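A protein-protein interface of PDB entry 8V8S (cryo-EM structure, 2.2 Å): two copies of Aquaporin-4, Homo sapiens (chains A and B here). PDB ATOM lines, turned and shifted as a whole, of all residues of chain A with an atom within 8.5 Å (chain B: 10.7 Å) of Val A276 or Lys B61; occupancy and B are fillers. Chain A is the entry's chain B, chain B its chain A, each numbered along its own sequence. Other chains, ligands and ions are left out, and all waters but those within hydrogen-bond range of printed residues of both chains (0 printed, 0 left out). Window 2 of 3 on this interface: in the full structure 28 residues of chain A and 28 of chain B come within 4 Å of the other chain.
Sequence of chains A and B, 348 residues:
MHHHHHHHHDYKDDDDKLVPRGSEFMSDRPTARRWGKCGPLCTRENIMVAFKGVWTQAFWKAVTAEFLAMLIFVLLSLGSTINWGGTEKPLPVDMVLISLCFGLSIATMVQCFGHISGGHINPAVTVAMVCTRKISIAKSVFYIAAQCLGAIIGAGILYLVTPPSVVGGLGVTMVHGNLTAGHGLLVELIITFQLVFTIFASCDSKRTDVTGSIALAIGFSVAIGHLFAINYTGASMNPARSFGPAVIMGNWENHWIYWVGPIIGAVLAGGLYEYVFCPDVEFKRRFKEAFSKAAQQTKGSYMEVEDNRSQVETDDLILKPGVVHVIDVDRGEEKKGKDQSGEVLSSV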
ATOM      1  N   PHE A 197       3.011  -0.771  -3.708  1.00  0.00           N
ATOM      2  CA  PHE A 197       2.980  -0.388  -2.300  1.00  0.00           C
ATOM      3  C   PHE A 197       1.599   0.115  -1.899  1.00  0.00           C
ATOM      4  O   PHE A 197       1.101  -0.213  -0.817  1.00  0.00           O
ATOM      5  CB  PHE A 197       4.043   0.675  -2.023  1.00  0.00           C
ATOM      6  CG  PHE A 197       4.520   0.700  -0.600  1.00  0.00           C
ATOM      7  CD1 PHE A 197       3.789   1.347   0.381  1.00  0.00           C
ATOM      8  CD2 PHE A 197       5.702   0.073  -0.241  1.00  0.00           C
ATOM      9  CE1 PHE A 197       4.228   1.370   1.689  1.00  0.00           C
ATOM     10  CE2 PHE A 197       6.148   0.092   1.065  1.00  0.00           C
ATOM     11  CZ  PHE A 197       5.409   0.742   2.033  1.00  0.00           C
ATOM     12  N   LEU A 268      10.131  -5.522  -5.017  1.00  0.00           N
ATOM     13  CA  LEU A 268      10.719  -4.665  -3.992  1.00  0.00           C
ATOM     14  C   LEU A 268       9.643  -4.036  -3.116  1.00  0.00           C
ATOM     15  O   LEU A 268       9.809  -3.936  -1.894  1.00  0.00           O
ATOM     16  CB  LEU A 268      11.582  -3.585  -4.643  1.00  0.00           C
ATOM     17  CG  LEU A 268      13.099  -3.798  -4.624  1.00  0.00           C
ATOM     18  CD1 LEU A 268      13.677  -3.437  -3.265  1.00  0.00           C
ATOM     19  CD2 LEU A 268      13.456  -5.229  -4.997  1.00  0.00           C
ATOM     20  N   ALA A 269       8.535  -3.603  -3.721  1.00  0.00           N
ATOM     21  CA  ALA A 269       7.462  -2.979  -2.953  1.00  0.00           C
ATOM     22  C   ALA A 269       6.786  -3.984  -2.028  1.00  0.00           C
ATOM     23  O   ALA A 269       6.539  -3.691  -0.852  1.00  0.00           O
ATOM     24  CB  ALA A 269       6.440  -2.346  -3.897  1.00  0.00           C
ATOM     25  N   GLY A 270       6.474  -5.174  -2.544  1.00  0.00           N
ATOM     26  CA  GLY A 270       5.808  -6.172  -1.724  1.00  0.00           C
ATOM     27  C   GLY A 270       6.679  -6.676  -0.589  1.00  0.00           C
ATOM     28  O   GLY A 270       6.204  -6.857   0.535  1.00  0.00           O
ATOM     29  N   GLY A 271       7.962  -6.914  -0.867  1.00  0.00           N
ATOM     30  CA  GLY A 271       8.859  -7.376   0.178  1.00  0.00           C
ATOM     31  C   GLY A 271       9.091  -6.335   1.257  1.00  0.00           C
ATOM     32  O   GLY A 271       9.139  -6.663   2.446  1.00  0.00           O
ATOM     33  N   LEU A 272       9.243  -5.069   0.861  1.00  0.00           N
ATOM     34  CA  LEU A 272       9.470  -4.010   1.838  1.00  0.00           C
ATOM     35  C   LEU A 272       8.275  -3.848   2.767  1.00  0.00           C
ATOM     36  O   LEU A 272       8.439  -3.683   3.980  1.00  0.00           O
ATOM     37  CB  LEU A 272       9.773  -2.693   1.123  1.00  0.00           C
ATOM     38  CG  LEU A 272      10.957  -1.878   1.647  1.00  0.00           C
ATOM     39  CD1 LEU A 272      12.189  -2.756   1.808  1.00  0.00           C
ATOM     40  CD2 LEU A 272      11.247  -0.704   0.725  1.00  0.00           C
ATOM     41  N   TYR A 273       7.060  -3.886   2.216  1.00  0.00           N
ATOM     42  CA  TYR A 273       5.869  -3.723   3.043  1.00  0.00           C
ATOM     43  C   TYR A 273       5.653  -4.930   3.948  1.00  0.00           C
ATOM     44  O   TYR A 273       5.427  -4.783   5.154  1.00  0.00           O
ATOM     45  CB  TYR A 273       4.645  -3.487   2.157  1.00  0.00           C
ATOM     46  CG  TYR A 273       3.404  -3.087   2.922  1.00  0.00           C
ATOM     47  CD1 TYR A 273       3.132  -1.755   3.193  1.00  0.00           C
ATOM     48  CD2 TYR A 273       2.506  -4.046   3.377  1.00  0.00           C
ATOM     49  CE1 TYR A 273       2.002  -1.385   3.893  1.00  0.00           C
ATOM     50  CE2 TYR A 273       1.373  -3.686   4.080  1.00  0.00           C
ATOM     51  CZ  TYR A 273       1.125  -2.355   4.334  1.00  0.00           C
ATOM     52  OH  TYR A 273      -0.002  -1.991   5.032  1.00  0.00           O
ATOM     53  N   GLU A 274       5.725  -6.135   3.381  1.00  0.00           N
ATOM     54  CA  GLU A 274       5.348  -7.333   4.121  1.00  0.00           C
ATOM     55  C   GLU A 274       6.412  -7.775   5.119  1.00  0.00           C
ATOM     56  O   GLU A 274       6.074  -8.378   6.142  1.00  0.00           O
ATOM     57  CB  GLU A 274       5.047  -8.476   3.148  1.00  0.00           C
ATOM     58  CG  GLU A 274       3.739  -8.319   2.395  1.00  0.00           C
ATOM     59  CD  GLU A 274       2.528  -8.401   3.304  1.00  0.00           C
ATOM     60  OE1 GLU A 274       2.406  -9.400   4.044  1.00  0.00           O
ATOM     61  OE2 GLU A 274       1.698  -7.468   3.280  1.00  0.00           O
ATOM     62  N   TYR A 275       7.688  -7.497   4.850  1.00  0.00           N
ATOM     63  CA  TYR A 275       8.772  -8.053   5.647  1.00  0.00           C
ATOM     64  C   TYR A 275       9.626  -7.015   6.361  1.00  0.00           C
ATOM     65  O   TYR A 275      10.504  -7.397   7.143  1.00  0.00           O
ATOM     66  CB  TYR A 275       9.676  -8.929   4.769  1.00  0.00           C
ATOM     67  CG  TYR A 275       8.972 -10.120   4.162  1.00  0.00           C
ATOM     68  CD1 TYR A 275       7.899 -10.719   4.808  1.00  0.00           C
ATOM     69  CD2 TYR A 275       9.376 -10.641   2.941  1.00  0.00           C
ATOM     70  CE1 TYR A 275       7.251 -11.806   4.258  1.00  0.00           C
ATOM     71  CE2 TYR A 275       8.734 -11.728   2.383  1.00  0.00           C
ATOM     72  CZ  TYR A 275       7.672 -12.307   3.045  1.00  0.00           C
ATOM     73  OH  TYR A 275       7.027 -13.389   2.496  1.00  0.00           O
ATOM     74  N   VAL A 276       9.406  -5.722   6.123  1.00  0.00           N
ATOM     75  CA  VAL A 276      10.218  -4.692   6.762  1.00  0.00           C
ATOM     76  C   VAL A 276       9.326  -3.713   7.514  1.00  0.00           C
ATOM     77  O   VAL A 276       9.530  -3.462   8.707  1.00  0.00           O
ATOM     78  CB  VAL A 276      11.094  -3.952   5.734  1.00  0.00           C
ATOM     79  CG1 VAL A 276      11.903  -2.860   6.414  1.00  0.00           C
ATOM     80  CG2 VAL A 276      12.009  -4.930   5.013  1.00  0.00           C
ATOM     81  N   PHE A 277       8.330  -3.155   6.825  1.00  0.00           N
ATOM     82  CA  PHE A 277       7.518  -2.101   7.423  1.00  0.00           C
ATOM     83  C   PHE A 277       6.422  -2.666   8.318  1.00  0.00           C
ATOM     84  O   PHE A 277       6.257  -2.228   9.461  1.00  0.00           O
ATOM     85  CB  PHE A 277       6.916  -1.218   6.328  1.00  0.00           C
ATOM     86  CG  PHE A 277       7.862  -0.175   5.805  1.00  0.00           C
ATOM     87  CD1 PHE A 277       8.335   0.827   6.636  1.00  0.00           C
ATOM     88  CD2 PHE A 277       8.280  -0.198   4.486  1.00  0.00           C
ATOM     89  CE1 PHE A 277       9.207   1.787   6.160  1.00  0.00           C
ATOM     90  CE2 PHE A 277       9.152   0.760   4.006  1.00  0.00           C
ATOM     91  CZ  PHE A 277       9.615   1.754   4.843  1.00  0.00           C
ATOM     92  N   CYS A 278       5.660  -3.637   7.818  1.00  0.00           N
ATOM     93  CA  CYS A 278       4.556  -4.243   8.563  1.00  0.00           C
ATOM     94  C   CYS A 278       4.686  -5.761   8.516  1.00  0.00           C
ATOM     95  O   CYS A 278       3.948  -6.439   7.791  1.00  0.00           O
ATOM     96  CB  CYS A 278       3.208  -3.787   8.007  1.00  0.00           C
ATOM     97  SG  CYS A 278       2.987  -1.994   7.962  1.00  0.00           S
ATOM     98  N   PRO A 279       5.622  -6.333   9.288  1.00  0.00           N
ATOM     99  CA  PRO A 279       5.803  -7.788   9.317  1.00  0.00           C
ATOM    100  C   PRO A 279       4.779  -8.495  10.200  1.00  0.00           C
ATOM    101  O   PRO A 279       3.613  -8.100  10.208  1.00  0.00           O
ATOM    102  CB  PRO A 279       7.212  -7.944   9.887  1.00  0.00           C
ATOM    103  CG  PRO A 279       7.364  -6.774  10.789  1.00  0.00           C
ATOM    104  CD  PRO A 279       6.597  -5.642  10.151  1.00  0.00           C
ATOM    105  N   GLN B  57      12.860  -1.308  16.073  1.00  0.00           N
ATOM    106  CA  GLN B  57      12.432  -0.020  16.606  1.00  0.00           C
ATOM    107  C   GLN B  57      11.409   0.643  15.692  1.00  0.00           C
ATOM    108  O   GLN B  57      11.655   0.832  14.501  1.00  0.00           O
ATOM    109  CB  GLN B  57      13.637   0.903  16.802  1.00  0.00           C
ATOM    110  CG  GLN B  57      13.272   2.321  17.217  1.00  0.00           C
ATOM    111  CD  GLN B  57      12.675   2.387  18.608  1.00  0.00           C
ATOM    112  OE1 GLN B  57      11.572   2.901  18.799  1.00  0.00           O
ATOM    113  NE2 GLN B  57      13.400   1.864  19.590  1.00  0.00           N
ATOM    114  N   ALA B  58      10.253   0.995  16.261  1.00  0.00           N
ATOM    115  CA  ALA B  58       9.215   1.653  15.478  1.00  0.00           C
ATOM    116  C   ALA B  58       9.631   3.055  15.050  1.00  0.00           C
ATOM    117  O   ALA B  58       9.157   3.552  14.023  1.00  0.00           O
ATOM    118  CB  ALA B  58       7.909   1.706  16.271  1.00  0.00           C
ATOM    119  N   PHE B  59      10.504   3.706  15.824  1.00  0.00           N
ATOM    120  CA  PHE B  59      10.950   5.050  15.468  1.00  0.00           C
ATOM    121  C   PHE B  59      11.760   5.046  14.177  1.00  0.00           C
ATOM    122  O   PHE B  59      11.568   5.910  13.315  1.00  0.00           O
ATOM    123  CB  PHE B  59      11.767   5.650  16.610  1.00  0.00           C
ATOM    124  CG  PHE B  59      12.305   7.020  16.314  1.00  0.00           C
ATOM    125  CD1 PHE B  59      11.461   8.039  15.908  1.00  0.00           C
ATOM    126  CD2 PHE B  59      13.658   7.288  16.438  1.00  0.00           C
ATOM    127  CE1 PHE B  59      11.956   9.297  15.631  1.00  0.00           C
ATOM    128  CE2 PHE B  59      14.158   8.545  16.164  1.00  0.00           C
ATOM    129  CZ  PHE B  59      13.306   9.553  15.761  1.00  0.00           C
ATOM    130  N   TRP B  60      12.676   4.085  14.027  1.00  0.00           N
ATOM    131  CA  TRP B  60      13.480   4.018  12.812  1.00  0.00           C
ATOM    132  C   TRP B  60      12.621   3.726  11.589  1.00  0.00           C
ATOM    133  O   TRP B  60      12.901   4.235  10.498  1.00  0.00           O
ATOM    134  CB  TRP B  60      14.579   2.966  12.962  1.00  0.00           C
ATOM    135  CG  TRP B  60      15.640   3.343  13.948  1.00  0.00           C
ATOM    136  CD1 TRP B  60      15.699   2.987  15.265  1.00  0.00           C
ATOM    137  CD2 TRP B  60      16.806   4.138  13.697  1.00  0.00           C
ATOM    138  NE1 TRP B  60      16.821   3.519  15.851  1.00  0.00           N
ATOM    139  CE2 TRP B  60      17.519   4.229  14.908  1.00  0.00           C
ATOM    140  CE3 TRP B  60      17.313   4.784  12.566  1.00  0.00           C
ATOM    141  CZ2 TRP B  60      18.712   4.940  15.022  1.00  0.00           C
ATOM    142  CZ3 TRP B  60      18.498   5.488  12.680  1.00  0.00           C
ATOM    143  CH2 TRP B  60      19.183   5.561  13.898  1.00  0.00           C
ATOM    144  N   LYS B  61      11.578   2.909  11.749  1.00  0.00           N
ATOM    145  CA  LYS B  61      10.676   2.642  10.634  1.00  0.00           C
ATOM    146  C   LYS B  61       9.872   3.880  10.254  1.00  0.00           C
ATOM    147  O   LYS B  61       9.548   4.069   9.077  1.00  0.00           O
ATOM    148  CB  LYS B  61       9.738   1.486  10.984  1.00  0.00           C
ATOM    149  CG  LYS B  61       9.953   0.240  10.142  1.00  0.00           C
ATOM    150  CD  LYS B  61       9.595  -1.020  10.915  1.00  0.00           C
ATOM    151  CE  LYS B  61       8.267  -0.875  11.638  1.00  0.00           C
ATOM    152  NZ  LYS B  61       7.945  -2.080  12.450  1.00  0.00           N
ATOM    153  N   ALA B  62       9.543   4.729  11.231  1.00  0.00           N
ATOM    154  CA  ALA B  62       8.804   5.949  10.928  1.00  0.00           C
ATOM    155  C   ALA B  62       9.680   6.964  10.204  1.00  0.00           C
ATOM    156  O   ALA B  62       9.210   7.668   9.304  1.00  0.00           O
ATOM    157  CB  ALA B  62       8.234   6.549  12.213  1.00  0.00           C
ATOM    158  N   VAL B  63      10.955   7.057  10.587  1.00  0.00           N
ATOM    159  CA  VAL B  63      11.865   7.983   9.918  1.00  0.00           C
ATOM    160  C   VAL B  63      12.138   7.524   8.492  1.00  0.00           C
ATOM    161  O   VAL B  63      12.182   8.338   7.561  1.00  0.00           O
ATOM    162  CB  VAL B  63      13.166   8.130  10.729  1.00  0.00           C
ATOM    163  CG1 VAL B  63      14.168   8.990   9.978  1.00  0.00           C
ATOM    164  CG2 VAL B  63      12.870   8.724  12.097  1.00  0.00           C
ATOM    165  N   THR B  64      12.324   6.216   8.296  1.00  0.00           N
ATOM    166  CA  THR B  64      12.530   5.686   6.952  1.00  0.00           C
ATOM    167  C   THR B  64      11.303   5.908   6.078  1.00  0.00           C
ATOM    168  O   THR B  64      11.427   6.252   4.896  1.00  0.00           O
ATOM    169  CB  THR B  64      12.877   4.199   7.024  1.00  0.00           C
ATOM    170  OG1 THR B  64      14.074   4.026   7.791  1.00  0.00           O
ATOM    171  CG2 THR B  64      13.090   3.630   5.631  1.00  0.00           C
ATOM    172  N   ALA B  65      10.107   5.720   6.642  1.00  0.00           N
ATOM    173  CA  ALA B  65       8.883   5.921   5.872  1.00  0.00           C
ATOM    174  C   ALA B  65       8.749   7.366   5.409  1.00  0.00           C
ATOM    175  O   ALA B  65       8.331   7.626   4.276  1.00  0.00           O
ATOM    176  CB  ALA B  65       7.668   5.506   6.700  1.00  0.00           C
ATOM    177  N   GLU B  66       9.090   8.322   6.278  1.00  0.00           N
ATOM    178  CA  GLU B  66       9.023   9.729   5.895  1.00  0.00           C
ATOM    179  C   GLU B  66      10.016  10.048   4.783  1.00  0.00           C
ATOM    180  O   GLU B  66       9.699  10.807   3.859  1.00  0.00           O
ATOM    181  CB  GLU B  66       9.277  10.619   7.111  1.00  0.00           C
ATOM    182  CG  GLU B  66       8.036  10.909   7.942  1.00  0.00           C
ATOM    183  CD  GLU B  66       7.090  11.885   7.270  1.00  0.00           C
ATOM    184  OE1 GLU B  66       7.572  12.802   6.573  1.00  0.00           O
ATOM    185  OE2 GLU B  66       5.861  11.739   7.443  1.00  0.00           O
ATOM    186  N   PHE B  67      11.225   9.487   4.862  1.00  0.00           N
ATOM    187  CA  PHE B  67      12.220   9.707   3.816  1.00  0.00           C
ATOM    188  C   PHE B  67      11.750   9.136   2.483  1.00  0.00           C
ATOM    189  O   PHE B  67      11.877   9.783   1.437  1.00  0.00           O
ATOM    190  CB  PHE B  67      13.556   9.086   4.232  1.00  0.00           C
ATOM    191  CG  PHE B  67      14.545   8.955   3.106  1.00  0.00           C
ATOM    192  CD1 PHE B  67      15.374  10.011   2.770  1.00  0.00           C
ATOM    193  CD2 PHE B  67      14.656   7.771   2.392  1.00  0.00           C
ATOM    194  CE1 PHE B  67      16.286   9.895   1.738  1.00  0.00           C
ATOM    195  CE2 PHE B  67      15.565   7.650   1.359  1.00  0.00           C
ATOM    196  CZ  PHE B  67      16.382   8.713   1.033  1.00  0.00           C
ATOM    197  N   LEU B  68      11.207   7.917   2.502  1.00  0.00           N
ATOM    198  CA  LEU B  68      10.785   7.277   1.260  1.00  0.00           C
ATOM    199  C   LEU B  68       9.552   7.955   0.672  1.00  0.00           C
ATOM    200  O   LEU B  68       9.447   8.110  -0.550  1.00  0.00           O
ATOM    201  CB  LEU B  68      10.526   5.790   1.499  1.00  0.00           C
ATOM    202  CG  LEU B  68      10.106   4.955   0.289  1.00  0.00           C
ATOM    203  CD1 LEU B  68      11.194   4.956  -0.769  1.00  0.00           C
ATOM    204  CD2 LEU B  68       9.775   3.533   0.713  1.00  0.00           C
ATOM    205  N   ALA B  69       8.607   8.360   1.525  1.00  0.00           N
ATOM    206  CA  ALA B  69       7.407   9.030   1.031  1.00  0.00           C
ATOM    207  C   ALA B  69       7.748  10.358   0.372  1.00  0.00           C
ATOM    208  O   ALA B  69       7.171  10.715  -0.663  1.00  0.00           O
ATOM    209  CB  ALA B  69       6.411   9.237   2.170  1.00  0.00           C
ATOM    210  N   CYS B 112      -0.339   5.386   1.649  1.00  0.00           N
ATOM    211  CA  CYS B 112       0.719   4.383   1.733  1.00  0.00           C
ATOM    212  C   CYS B 112       1.388   4.373   3.103  1.00  0.00           C
ATOM    213  O   CYS B 112       1.672   3.303   3.651  1.00  0.00           O
ATOM    214  CB  CYS B 112       1.760   4.634   0.643  1.00  0.00           C
ATOM    215  SG  CYS B 112       1.266   4.123  -1.012  1.00  0.00           S
ATOM    216  N   PHE B 113       1.653   5.552   3.670  1.00  0.00           N
ATOM    217  CA  PHE B 113       2.506   5.670   4.847  1.00  0.00           C
ATOM    218  C   PHE B 113       1.816   6.329   6.035  1.00  0.00           C
ATOM    219  O   PHE B 113       2.499   6.739   6.981  1.00  0.00           O
ATOM    220  CB  PHE B 113       3.777   6.449   4.498  1.00  0.00           C
ATOM    221  CG  PHE B 113       4.688   5.731   3.543  1.00  0.00           C
ATOM    222  CD1 PHE B 113       5.449   4.655   3.966  1.00  0.00           C
ATOM    223  CD2 PHE B 113       4.781   6.134   2.221  1.00  0.00           C
ATOM    224  CE1 PHE B 113       6.288   3.996   3.090  1.00  0.00           C
ATOM    225  CE2 PHE B 113       5.619   5.477   1.340  1.00  0.00           C
ATOM    226  CZ  PHE B 113       6.373   4.407   1.775  1.00  0.00           C
ATOM    227  N   GLY B 114       0.487   6.448   6.017  1.00  0.00           N
ATOM    228  CA  GLY B 114      -0.199   7.103   7.118  1.00  0.00           C
ATOM    229  C   GLY B 114      -0.105   6.335   8.424  1.00  0.00           C
ATOM    230  O   GLY B 114       0.048   6.929   9.494  1.00  0.00           O
ATOM    231  N   HIS B 115      -0.193   5.008   8.356  1.00  0.00           N
ATOM    232  CA  HIS B 115      -0.203   4.179   9.555  1.00  0.00           C
ATOM    233  C   HIS B 115       1.191   3.830  10.059  1.00  0.00           C
ATOM    234  O   HIS B 115       1.306   3.164  11.092  1.00  0.00           O
ATOM    235  CB  HIS B 115      -0.987   2.887   9.297  1.00  0.00           C
ATOM    236  CG  HIS B 115      -0.342   1.972   8.302  1.00  0.00           C
ATOM    237  ND1 HIS B 115       0.057   2.392   7.053  1.00  0.00           N
ATOM    238  CD2 HIS B 115      -0.029   0.657   8.375  1.00  0.00           C
ATOM    239  CE1 HIS B 115       0.589   1.374   6.397  1.00  0.00           C
ATOM    240  NE2 HIS B 115       0.549   0.310   7.178  1.00  0.00           N
ATOM    241  N   ILE B 116       2.245   4.252   9.369  1.00  0.00           N
ATOM    242  CA  ILE B 116       3.612   3.916   9.748  1.00  0.00           C
ATOM    243  C   ILE B 116       4.303   5.077  10.451  1.00  0.00           C
ATOM    244  O   ILE B 116       4.897   4.904  11.514  1.00  0.00           O
ATOM    245  CB  ILE B 116       4.411   3.456   8.508  1.00  0.00           C
ATOM    246  CG1 ILE B 116       3.733   2.250   7.856  1.00  0.00           C
ATOM    247  CG2 ILE B 116       5.841   3.115   8.897  1.00  0.00           C
ATOM    248  CD1 ILE B 116       4.325   1.861   6.522  1.00  0.00           C
ATOM    249  N   SER B 117       4.229   6.274   9.871  1.00  0.00           N
ATOM    250  CA  SER B 117       4.873   7.448  10.438  1.00  0.00           C
ATOM    251  C   SER B 117       3.924   8.613  10.678  1.00  0.00           C
ATOM    252  O   SER B 117       4.352   9.628  11.239  1.00  0.00           O
ATOM    253  CB  SER B 117       6.017   7.924   9.529  1.00  0.00           C
ATOM    254  OG  SER B 117       5.517   8.450   8.312  1.00  0.00           O
ATOM    255  N   GLY B 118       2.661   8.501  10.277  1.00  0.00           N
ATOM    256  CA  GLY B 118       1.721   9.593  10.337  1.00  0.00           C
ATOM    257  C   GLY B 118       1.531  10.320   9.024  1.00  0.00           C
ATOM    258  O   GLY B 118       0.546  11.051   8.872  1.00  0.00           O
ATOM    259  N   GLY B 119       2.445  10.134   8.073  1.00  0.00           N
ATOM    260  CA  GLY B 119       2.324  10.724   6.756  1.00  0.00           C
ATOM    261  C   GLY B 119       2.366  12.237   6.736  1.00  0.00           C
ATOM    262  O   GLY B 119       1.543  12.873   6.072  1.00  0.00           O
ATOM    263  N   LYS B 139      11.490  13.649  17.791  1.00  0.00           N
ATOM    264  CA  LYS B 139      10.888  13.096  16.584  1.00  0.00           C
ATOM    265  C   LYS B 139      10.878  14.106  15.443  1.00  0.00           C
ATOM    266  O   LYS B 139      10.983  13.718  14.275  1.00  0.00           O
ATOM    267  CB  LYS B 139       9.466  12.617  16.878  1.00  0.00           C
ATOM    268  CG  LYS B 139       9.154  11.229  16.346  1.00  0.00           C
ATOM    269  CD  LYS B 139       7.695  11.099  15.941  1.00  0.00           C
ATOM    270  CE  LYS B 139       7.413   9.734  15.336  1.00  0.00           C
ATOM    271  NZ  LYS B 139       6.000   9.314  15.541  1.00  0.00           N
ATOM    272  N   PHE B 142      14.384  14.540  13.498  1.00  0.00           N
ATOM    273  CA  PHE B 142      14.615  13.414  12.602  1.00  0.00           C
ATOM    274  C   PHE B 142      13.617  13.394  11.453  1.00  0.00           C
ATOM    275  O   PHE B 142      13.949  12.934  10.355  1.00  0.00           O
ATOM    276  CB  PHE B 142      14.552  12.099  13.379  1.00  0.00           C
ATOM    277  CG  PHE B 142      15.801  11.795  14.154  1.00  0.00           C
ATOM    278  CD1 PHE B 142      16.882  11.187  13.539  1.00  0.00           C
ATOM    279  CD2 PHE B 142      15.895  12.117  15.496  1.00  0.00           C
ATOM    280  CE1 PHE B 142      18.033  10.906  14.249  1.00  0.00           C
ATOM    281  CE2 PHE B 142      17.044  11.840  16.212  1.00  0.00           C
ATOM    282  CZ  PHE B 142      18.113  11.232  15.587  1.00  0.00           C
ATOM    283  N   TYR B 143      12.398  13.883  11.687  1.00  0.00           N
ATOM    284  CA  TYR B 143      11.398  13.941  10.626  1.00  0.00           C
ATOM    285  C   TYR B 143      11.778  14.973   9.571  1.00  0.00           C
ATOM    286  O   TYR B 143      11.686  14.708   8.367  1.00  0.00           O
ATOM    287  CB  TYR B 143      10.028  14.262  11.221  1.00  0.00           C
ATOM    288  CG  TYR B 143       9.146  13.054  11.439  1.00  0.00           C
ATOM    289  CD1 TYR B 143       7.796  13.092  11.123  1.00  0.00           C
ATOM    290  CD2 TYR B 143       9.665  11.880  11.968  1.00  0.00           C
ATOM    291  CE1 TYR B 143       6.986  11.993  11.325  1.00  0.00           C
ATOM    292  CE2 TYR B 143       8.863  10.777  12.172  1.00  0.00           C
ATOM    293  CZ  TYR B 143       7.525  10.840  11.849  1.00  0.00           C
ATOM    294  OH  TYR B 143       6.721   9.742  12.052  1.00  0.00           O
ATOM    295  N   ALA B 146      14.831  13.869   7.464  1.00  0.00           N
ATOM    296  CA  ALA B 146      14.445  12.848   6.493  1.00  0.00           C
ATOM    297  C   ALA B 146      13.673  13.458   5.330  1.00  0.00           C
ATOM    298  O   ALA B 146      13.858  13.055   4.176  1.00  0.00           O
ATOM    299  CB  ALA B 146      13.617  11.760   7.176  1.00  0.00           C
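Of the printed residues of chain B, Phe A197 touches Cys B112 and Phe B113. No residue of chain B comes within 4 Å of Leu A272. Of the printed residues of chain B, Tyr A273 touches His B115 (3.2 Å). Val A276 touches just one residue of chain B: Lys B61. Phe A277 touches just one residue of chain B: Lys B61. Cys A278 touches just one residue of chain B: His B115 (3.4 Å). Of chain A, only Val A276 and Phe A277 come within 4 Å of Lys B61. Val B63 touches none of the printed residues of chain A. Of the printed residues of chain A, Cys B112 touches Phe A197. Of the printed residues of chain A, Phe B113 touches Phe A197 (3.5 Å). Of the printed residues of chain A, His B115 touches Tyr A273 (3.2 Å) and Cys A278 (3.4 Å). The nearest residue of chain B that does not touch Val A276 is Thr B64 (6.6 Å). The nearest residue of chain A that does not touch Lys B61 is Pro A279 (4.4 Å).
Among the printed residues, pairs that only touch across the chains: Phe A197 with Cys B112 (3.8 Å), Phe A197 with Phe B113 (3.5 Å) and Val A276 with Lys B61 (3.3 Å).
The side-chain amino group (NZ) of Lys B61 sits close to the backbone carbonyl oxygen (O) of Phe A277. OH of Tyr A273 is in hydrogen-bond range of NE2 of His B115 (3.2 Å). NE2 of His B115 lies within hydrogen-bond range of SG of Cys A278 (3.4 Å).
Of the 25 printed residues of chain B, 4 touch a printed residue of chain A. Printed residues of chain B that touch a printed residue of chain A: Lys B61, Cys B112, Phe B113 and His B115. Hydrophobic or aromatic side chains of chain B that line the printed part of chain A: Phe B113 and His B115.
The backbone carbonyl oxygen (O) of Tyr A273 lies within hydrogen-bond range of the backbone NH (N) of Cys A278 (2.9 Å). The backbone carbonyl oxygen of Leu A272 sits at hydrogen-bond distance from the backbone NH of Phe A277, at 2.9 Å.
No position is printed for both chains. Of the 6 pairs that touch across the chains among the printed residues, none has its exchanged pair printed and touching as well.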
